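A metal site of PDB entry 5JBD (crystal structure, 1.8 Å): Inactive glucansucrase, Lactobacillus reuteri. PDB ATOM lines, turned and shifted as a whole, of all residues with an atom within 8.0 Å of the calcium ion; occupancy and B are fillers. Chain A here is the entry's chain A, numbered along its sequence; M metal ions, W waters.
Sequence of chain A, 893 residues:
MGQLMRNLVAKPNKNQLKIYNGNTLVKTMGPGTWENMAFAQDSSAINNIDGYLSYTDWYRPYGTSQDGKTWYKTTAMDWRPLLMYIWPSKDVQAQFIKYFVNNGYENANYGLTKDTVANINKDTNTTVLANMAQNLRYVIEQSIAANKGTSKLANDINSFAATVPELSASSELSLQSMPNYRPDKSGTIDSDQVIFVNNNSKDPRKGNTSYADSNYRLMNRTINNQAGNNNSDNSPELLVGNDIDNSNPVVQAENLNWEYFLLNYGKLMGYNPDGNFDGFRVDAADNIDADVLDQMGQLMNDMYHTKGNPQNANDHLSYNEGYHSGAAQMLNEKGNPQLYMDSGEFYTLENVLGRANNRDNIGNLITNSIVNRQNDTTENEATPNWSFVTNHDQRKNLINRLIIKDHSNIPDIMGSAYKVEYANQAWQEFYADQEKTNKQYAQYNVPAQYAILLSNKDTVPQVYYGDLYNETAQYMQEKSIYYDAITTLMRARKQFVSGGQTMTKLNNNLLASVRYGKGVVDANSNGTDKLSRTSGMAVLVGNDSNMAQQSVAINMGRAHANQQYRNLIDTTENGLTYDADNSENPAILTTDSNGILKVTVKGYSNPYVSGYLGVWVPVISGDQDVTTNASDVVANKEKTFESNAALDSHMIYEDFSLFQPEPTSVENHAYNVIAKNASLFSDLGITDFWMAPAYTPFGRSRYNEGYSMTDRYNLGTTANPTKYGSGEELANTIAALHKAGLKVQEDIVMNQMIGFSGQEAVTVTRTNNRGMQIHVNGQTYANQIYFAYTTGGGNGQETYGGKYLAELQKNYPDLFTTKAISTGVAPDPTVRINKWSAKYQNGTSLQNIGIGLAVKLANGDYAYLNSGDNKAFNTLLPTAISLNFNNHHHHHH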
ATOM      1  N   LEU A 218     -24.535   3.227  -8.439  1.00  0.00           N
ATOM      2  CA  LEU A 218     -25.608   4.106  -7.966  1.00  0.00           C
ATOM      3  C   LEU A 218     -25.191   4.500  -6.558  1.00  0.00           C
ATOM      4  O   LEU A 218     -25.169   3.664  -5.665  1.00  0.00           O
ATOM      5  CB  LEU A 218     -26.954   3.394  -7.948  1.00  0.00           C
ATOM      6  CG  LEU A 218     -27.448   2.842  -9.290  1.00  0.00           C
ATOM      7  CD1 LEU A 218     -28.868   2.304  -9.180  1.00  0.00           C
ATOM      8  CD2 LEU A 218     -27.370   3.875 -10.420  1.00  0.00           C
ATOM      9  N   MET A 219     -24.759   5.754  -6.398  1.00  0.00           N
ATOM     10  CA  MET A 219     -24.231   6.205  -5.113  1.00  0.00           C
ATOM     11  C   MET A 219     -25.309   6.932  -4.300  1.00  0.00           C
ATOM     12  O   MET A 219     -26.215   7.520  -4.862  1.00  0.00           O
ATOM     13  CB  MET A 219     -23.039   7.123  -5.310  1.00  0.00           C
ATOM     14  CG  MET A 219     -21.850   6.396  -5.946  1.00  0.00           C
ATOM     15  SD  MET A 219     -20.400   7.432  -6.020  1.00  0.00           S
ATOM     16  CE  MET A 219     -19.876   7.543  -4.332  1.00  0.00           C
ATOM     17  N   ASN A 220     -25.193   6.844  -2.988  1.00  0.00           N
ATOM     18  CA  ASN A 220     -26.055   7.550  -2.043  1.00  0.00           C
ATOM     19  C   ASN A 220     -27.502   7.050  -2.063  1.00  0.00           C
ATOM     20  O   ASN A 220     -28.413   7.768  -1.673  1.00  0.00           O
ATOM     21  CB  ASN A 220     -26.004   9.089  -2.275  1.00  0.00           C
ATOM     22  CG  ASN A 220     -24.591   9.616  -2.391  1.00  0.00           C
ATOM     23  OD1 ASN A 220     -23.800   9.567  -1.447  1.00  0.00           O
ATOM     24  ND2 ASN A 220     -24.247  10.123  -3.566  1.00  0.00           N
ATOM     25  N   THR A 222     -29.070   5.482  -0.031  1.00  0.00           N
ATOM     26  CA  THR A 222     -28.883   5.182   1.384  1.00  0.00           C
ATOM     27  C   THR A 222     -30.144   5.564   2.140  1.00  0.00           C
ATOM     28  O   THR A 222     -30.749   6.597   1.847  1.00  0.00           O
ATOM     29  CB  THR A 222     -27.725   6.010   1.937  1.00  0.00           C
ATOM     30  OG1 THR A 222     -27.843   7.379   1.509  1.00  0.00           O
ATOM     31  CG2 THR A 222     -26.382   5.427   1.413  1.00  0.00           C
ATOM     32  N   PRO A 236     -24.169   9.751   3.503  1.00  0.00           N
ATOM     33  CA  PRO A 236     -23.167   9.633   2.428  1.00  0.00           C
ATOM     34  C   PRO A 236     -22.801   8.209   2.035  1.00  0.00           C
ATOM     35  O   PRO A 236     -22.815   7.283   2.866  1.00  0.00           O
ATOM     36  CB  PRO A 236     -21.936  10.346   3.031  1.00  0.00           C
ATOM     37  CG  PRO A 236     -22.064  10.118   4.499  1.00  0.00           C
ATOM     38  CD  PRO A 236     -23.552  10.184   4.781  1.00  0.00           C
ATOM     39  N   GLU A 237     -22.443   8.048   0.762  1.00  0.00           N
ATOM     40  CA  GLU A 237     -21.973   6.761   0.244  1.00  0.00           C
ATOM     41  C   GLU A 237     -20.590   6.403   0.812  1.00  0.00           C
ATOM     42  O   GLU A 237     -20.317   5.222   1.085  1.00  0.00           O
ATOM     43  CB  GLU A 237     -21.889   6.784  -1.277  1.00  0.00           C
ATOM     44  CG  GLU A 237     -21.497   5.447  -1.925  1.00  0.00           C
ATOM     45  CD  GLU A 237     -22.489   4.354  -1.608  1.00  0.00           C
ATOM     46  OE1 GLU A 237     -23.674   4.549  -1.962  1.00  0.00           O
ATOM     47  OE2 GLU A 237     -22.106   3.340  -0.974  1.00  0.00           O
ATOM     48  N   LEU A 238     -19.724   7.407   0.962  1.00  0.00           N
ATOM     49  CA  LEU A 238     -18.298   7.171   1.244  1.00  0.00           C
ATOM     50  C   LEU A 238     -17.895   7.468   2.686  1.00  0.00           C
ATOM     51  O   LEU A 238     -18.283   8.520   3.238  1.00  0.00           O
ATOM     52  CB  LEU A 238     -17.441   8.007   0.283  1.00  0.00           C
ATOM     53  CG  LEU A 238     -17.752   7.839  -1.209  1.00  0.00           C
ATOM     54  CD1 LEU A 238     -16.893   8.766  -2.057  1.00  0.00           C
ATOM     55  CD2 LEU A 238     -17.558   6.396  -1.666  1.00  0.00           C
ATOM     56  N   LEU A 239     -17.148   6.550   3.280  1.00  0.00           N
ATOM     57  CA  LEU A 239     -16.540   6.704   4.611  1.00  0.00           C
ATOM     58  C   LEU A 239     -15.014   6.689   4.505  1.00  0.00           C
ATOM     59  O   LEU A 239     -14.355   7.725   4.638  1.00  0.00           O
ATOM     60  CB  LEU A 239     -17.005   5.601   5.555  1.00  0.00           C
ATOM     61  CG  LEU A 239     -18.494   5.561   5.890  1.00  0.00           C
ATOM     62  CD1 LEU A 239     -18.821   4.344   6.746  1.00  0.00           C
ATOM     63  CD2 LEU A 239     -18.927   6.857   6.588  1.00  0.00           C
ATOM     64  N   VAL A 240     -14.457   5.505   4.227  1.00  0.00           N
ATOM     65  CA  VAL A 240     -12.994   5.305   4.169  1.00  0.00           C
ATOM     66  C   VAL A 240     -12.707   3.988   3.458  1.00  0.00           C
ATOM     67  O   VAL A 240     -13.543   3.066   3.473  1.00  0.00           O
ATOM     68  CB  VAL A 240     -12.360   5.323   5.587  1.00  0.00           C
ATOM     69  CG1 VAL A 240     -12.739   4.073   6.381  1.00  0.00           C
ATOM     70  CG2 VAL A 240     -10.842   5.477   5.507  1.00  0.00           C
ATOM     71  N   ASN A 242     -11.610   1.318   0.196  1.00  0.00           N
ATOM     72  CA  ASN A 242     -12.178   1.046  -1.106  1.00  0.00           C
ATOM     73  C   ASN A 242     -13.663   0.785  -0.916  1.00  0.00           C
ATOM     74  O   ASN A 242     -14.046  -0.249  -0.385  1.00  0.00           O
ATOM     75  CB  ASN A 242     -11.521  -0.172  -1.757  1.00  0.00           C
ATOM     76  CG  ASN A 242     -10.077   0.079  -2.142  1.00  0.00           C
ATOM     77  OD1 ASN A 242      -9.207   0.190  -1.287  1.00  0.00           O
ATOM     78  ND2 ASN A 242      -9.815   0.150  -3.446  1.00  0.00           N
ATOM     79  N   ASP A 243     -14.484   1.705  -1.413  1.00  0.00           N
ATOM     80  CA  ASP A 243     -15.936   1.630  -1.205  1.00  0.00           C
ATOM     81  C   ASP A 243     -16.552   0.621  -2.167  1.00  0.00           C
ATOM     82  O   ASP A 243     -16.411   0.748  -3.382  1.00  0.00           O
ATOM     83  CB  ASP A 243     -16.574   2.995  -1.400  1.00  0.00           C
ATOM     84  CG  ASP A 243     -18.002   3.059  -0.878  1.00  0.00           C
ATOM     85  OD1 ASP A 243     -18.161   3.061   0.349  1.00  0.00           O
ATOM     86  OD2 ASP A 243     -18.975   3.079  -1.666  1.00  0.00           O
ATOM     87  N   ILE A 244     -17.236  -0.387  -1.618  1.00  0.00           N
ATOM     88  CA  ILE A 244     -17.809  -1.450  -2.454  1.00  0.00           C
ATOM     89  C   ILE A 244     -19.112  -0.972  -3.106  1.00  0.00           C
ATOM     90  O   ILE A 244     -19.950  -0.349  -2.447  1.00  0.00           O
ATOM     91  CB  ILE A 244     -18.061  -2.725  -1.632  1.00  0.00           C
ATOM     92  CG1 ILE A 244     -16.749  -3.221  -0.990  1.00  0.00           C
ATOM     93  CG2 ILE A 244     -18.681  -3.812  -2.503  1.00  0.00           C
ATOM     94  CD1 ILE A 244     -15.638  -3.595  -1.959  1.00  0.00           C
ATOM     95  N   ASP A 245     -19.263  -1.245  -4.408  1.00  0.00           N
ATOM     96  CA  ASP A 245     -20.480  -0.881  -5.122  1.00  0.00           C
ATOM     97  C   ASP A 245     -21.615  -1.882  -4.820  1.00  0.00           C
ATOM     98  O   ASP A 245     -21.849  -2.834  -5.567  1.00  0.00           O
ATOM     99  CB  ASP A 245     -20.260  -0.769  -6.625  1.00  0.00           C
ATOM    100  CG  ASP A 245     -21.527  -0.360  -7.362  1.00  0.00           C
ATOM    101  OD1 ASP A 245     -22.512   0.081  -6.709  1.00  0.00           O
ATOM    102  OD2 ASP A 245     -21.560  -0.468  -8.609  1.00  0.00           O
ATOM    103  N   ASN A 246     -22.344  -1.594  -3.746  1.00  0.00           N
ATOM    104  CA  ASN A 246     -23.482  -2.422  -3.331  1.00  0.00           C
ATOM    105  C   ASN A 246     -24.775  -2.210  -4.167  1.00  0.00           C
ATOM    106  O   ASN A 246     -25.798  -2.819  -3.868  1.00  0.00           O
ATOM    107  CB  ASN A 246     -23.731  -2.255  -1.821  1.00  0.00           C
ATOM    108  CG  ASN A 246     -22.700  -3.003  -0.970  1.00  0.00           C
ATOM    109  OD1 ASN A 246     -22.683  -4.240  -0.940  1.00  0.00           O
ATOM    110  ND2 ASN A 246     -21.839  -2.280  -0.275  1.00  0.00           N
ATOM    111  N   ALA A 284     -22.136   0.096   9.185  1.00  0.00           N
ATOM    112  CA  ALA A 284     -22.309   1.173   8.180  1.00  0.00           C
ATOM    113  C   ALA A 284     -23.594   1.039   7.360  1.00  0.00           C
ATOM    114  O   ALA A 284     -23.633   1.282   6.147  1.00  0.00           O
ATOM    115  CB  ALA A 284     -21.079   1.216   7.266  1.00  0.00           C
ATOM    116  N   ASP A 286     -26.066   2.874   7.133  1.00  0.00           N
ATOM    117  CA  ASP A 286     -26.468   4.130   6.494  1.00  0.00           C
ATOM    118  C   ASP A 286     -25.614   4.520   5.284  1.00  0.00           C
ATOM    119  O   ASP A 286     -25.886   5.539   4.661  1.00  0.00           O
ATOM    120  CB  ASP A 286     -26.443   5.335   7.477  1.00  0.00           C
ATOM    121  CG  ASP A 286     -27.268   5.104   8.768  1.00  0.00           C
ATOM    122  OD1 ASP A 286     -28.127   4.207   8.797  1.00  0.00           O
ATOM    123  OD2 ASP A 286     -27.053   5.882   9.735  1.00  0.00           O
ATOM    124  N   ASN A 287     -24.576   3.744   4.964  1.00  0.00           N
ATOM    125  CA  ASN A 287     -23.601   4.155   3.953  1.00  0.00           C
ATOM    126  C   ASN A 287     -23.463   3.160   2.800  1.00  0.00           C
ATOM    127  O   ASN A 287     -22.497   3.212   2.055  1.00  0.00           O
ATOM    128  CB  ASN A 287     -22.258   4.369   4.634  1.00  0.00           C
ATOM    129  CG  ASN A 287     -22.375   5.205   5.904  1.00  0.00           C
ATOM    130  OD1 ASN A 287     -22.227   4.665   6.989  1.00  0.00           O
ATOM    131  ND2 ASN A 287     -22.672   6.493   5.766  1.00  0.00           N
ATOM    132  N   ILE A 288     -24.446   2.270   2.668  1.00  0.00           N
ATOM    133  CA  ILE A 288     -24.476   1.239   1.653  1.00  0.00           C
ATOM    134  C   ILE A 288     -25.865   1.280   0.989  1.00  0.00           C
ATOM    135  O   ILE A 288     -26.840   1.610   1.641  1.00  0.00           O
ATOM    136  CB  ILE A 288     -24.192  -0.162   2.253  1.00  0.00           C
ATOM    137  CG1 ILE A 288     -25.230  -0.547   3.323  1.00  0.00           C
ATOM    138  CG2 ILE A 288     -22.781  -0.204   2.846  1.00  0.00           C
ATOM    139  CD1 ILE A 288     -24.873  -1.794   4.139  1.00  0.00           C
ATOM    140  N   ASP A 289     -25.928   0.946  -0.293  1.00  0.00           N
ATOM    141  CA  ASP A 289     -27.195   0.797  -1.009  1.00  0.00           C
ATOM    142  C   ASP A 289     -28.156  -0.025  -0.148  1.00  0.00           C
ATOM    143  O   ASP A 289     -27.846  -1.159   0.228  1.00  0.00           O
ATOM    144  CB  ASP A 289     -26.965   0.159  -2.388  1.00  0.00           C
ATOM    145  CG  ASP A 289     -28.190   0.224  -3.291  1.00  0.00           C
ATOM    146  OD1 ASP A 289     -29.317  -0.019  -2.825  1.00  0.00           O
ATOM    147  OD2 ASP A 289     -28.028   0.495  -4.504  1.00  0.00           O
ATOM    148  N   MET A 750     -20.106  -4.663   4.778  1.00  0.00           N
ATOM    149  CA  MET A 750     -20.297  -4.533   3.318  1.00  0.00           C
ATOM    150  C   MET A 750     -19.803  -3.224   2.727  1.00  0.00           C
ATOM    151  O   MET A 750     -19.742  -3.108   1.507  1.00  0.00           O
ATOM    152  CB  MET A 750     -21.773  -4.752   2.935  1.00  0.00           C
ATOM    153  CG  MET A 750     -22.246  -6.192   3.087  1.00  0.00           C
ATOM    154  SD  MET A 750     -24.009  -6.477   2.751  1.00  0.00           S
ATOM    155  CE  MET A 750     -24.714  -6.039   4.357  1.00  0.00           C
ATOM    156  N   ASN A 751     -19.441  -2.239   3.548  1.00  0.00           N
ATOM    157  CA  ASN A 751     -19.184  -0.917   2.989  1.00  0.00           C
ATOM    158  C   ASN A 751     -17.858  -0.814   2.253  1.00  0.00           C
ATOM    159  O   ASN A 751     -17.821  -0.228   1.173  1.00  0.00           O
ATOM    160  CB  ASN A 751     -19.224   0.183   4.032  1.00  0.00           C
ATOM    161  CG  ASN A 751     -18.978   1.559   3.427  1.00  0.00           C
ATOM    162  OD1 ASN A 751     -19.790   2.069   2.637  1.00  0.00           O
ATOM    163  ND2 ASN A 751     -17.842   2.149   3.769  1.00  0.00           N
ATOM    164  N   GLN A 752     -16.783  -1.322   2.875  1.00  0.00           N
ATOM    165  CA  GLN A 752     -15.433  -1.162   2.332  1.00  0.00           C
ATOM    166  C   GLN A 752     -14.508  -2.350   2.595  1.00  0.00           C
ATOM    167  O   GLN A 752     -14.717  -3.101   3.537  1.00  0.00           O
ATOM    168  CB  GLN A 752     -14.749   0.095   2.878  1.00  0.00           C
ATOM    169  CG  GLN A 752     -14.117  -0.047   4.267  1.00  0.00           C
ATOM    170  CD  GLN A 752     -15.119  -0.058   5.414  1.00  0.00           C
ATOM    171  OE1 GLN A 752     -16.121   0.643   5.374  1.00  0.00           O
ATOM    172  NE2 GLN A 752     -14.842  -0.848   6.441  1.00  0.00           N
ATOM    173  N   ASN A 769     -17.655  13.138   0.272  1.00  0.00           N
ATOM    174  CA  ASN A 769     -18.168  11.823   0.671  1.00  0.00           C
ATOM    175  C   ASN A 769     -19.488  11.388   0.002  1.00  0.00           C
ATOM    176  O   ASN A 769     -19.954  10.277   0.228  1.00  0.00           O
ATOM    177  CB  ASN A 769     -18.267  11.707   2.190  1.00  0.00           C
ATOM    178  CG  ASN A 769     -19.271  12.665   2.803  1.00  0.00           C
ATOM    179  OD1 ASN A 769     -19.862  13.501   2.126  1.00  0.00           O
ATOM    180  ND2 ASN A 769     -19.419  12.580   4.117  1.00  0.00           N
ATOM    181  N   ASN A 842     -16.997   1.790  -5.944  1.00  0.00           N
ATOM    182  CA  ASN A 842     -17.441   3.160  -6.219  1.00  0.00           C
ATOM    183  C   ASN A 842     -16.282   4.150  -6.245  1.00  0.00           C
ATOM    184  O   ASN A 842     -16.334   5.138  -6.963  1.00  0.00           O
ATOM    185  CB  ASN A 842     -18.422   3.654  -5.135  1.00  0.00           C
ATOM    186  CG  ASN A 842     -19.791   2.998  -5.218  1.00  0.00           C
ATOM    187  OD1 ASN A 842     -20.431   2.744  -4.172  1.00  0.00           O
ATOM    188  ND2 ASN A 842     -20.258   2.732  -6.419  1.00  0.00           N
HETATM  189 CA    CA M   1     -20.547   2.943   0.678  1.00  0.00          CA
HETATM  190  O   HOH W   1     -20.377   0.628   0.062  1.00  0.00           O
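The backbone carbonyl oxygen (O) of Asn 751 is in hydrogen-bond range of the backbone NH (N) of Ile 244 (2.9 Å). The side-chain amide nitrogen (ND2) of Asn 751 lies within hydrogen-bond range of the side-chain amide oxygen (OE1) of Gln 752 (2.8 Å). The backbone NH (N) of Asn 220 lies within hydrogen-bond range of the side-chain carboxylate (OE1) of Glu 237, 2.9 Å away. The backbone NH (N) of Glu 237 lies within hydrogen-bond range of the backbone carbonyl oxygen (O) of Asn 769, 3.4 Å away. ND2 of Asn 287 is in hydrogen-bond range of O of Pro 236, at 3.0 Å. O of Asp 243 sits at hydrogen-bond distance from N of Asn 842 (2.8 Å).
Of the 24 residues printed, 4 come within 4 Å of the calcium ion. The nearest printed residue that does not touch the calcium ion is Ile 288 (4.4 Å).
OD1 of Asn 751 binds the calcium ion (2.3 Å). OE2 of Glu 237 binds the calcium ion (2.3 Å). The calcium ion is bound by O of Glu 237, at 2.3 Å. The calcium ion is bound by water W1 (2.4 Å). O of Asn 287 binds the calcium ion, at 2.4 Å. OD1 of Asp 243 is bound to the calcium ion, at 2.4 Å. OD2 of Asp 243 is bound to the calcium ion. The calcium ion has seven donor atoms within binding distance.
Water W1 lies within hydrogen-bond range of O of Ile 244 (2.7 Å), O of Asn 751 (2.9 Å) and ND2 of Asn 246 (3.3 Å).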
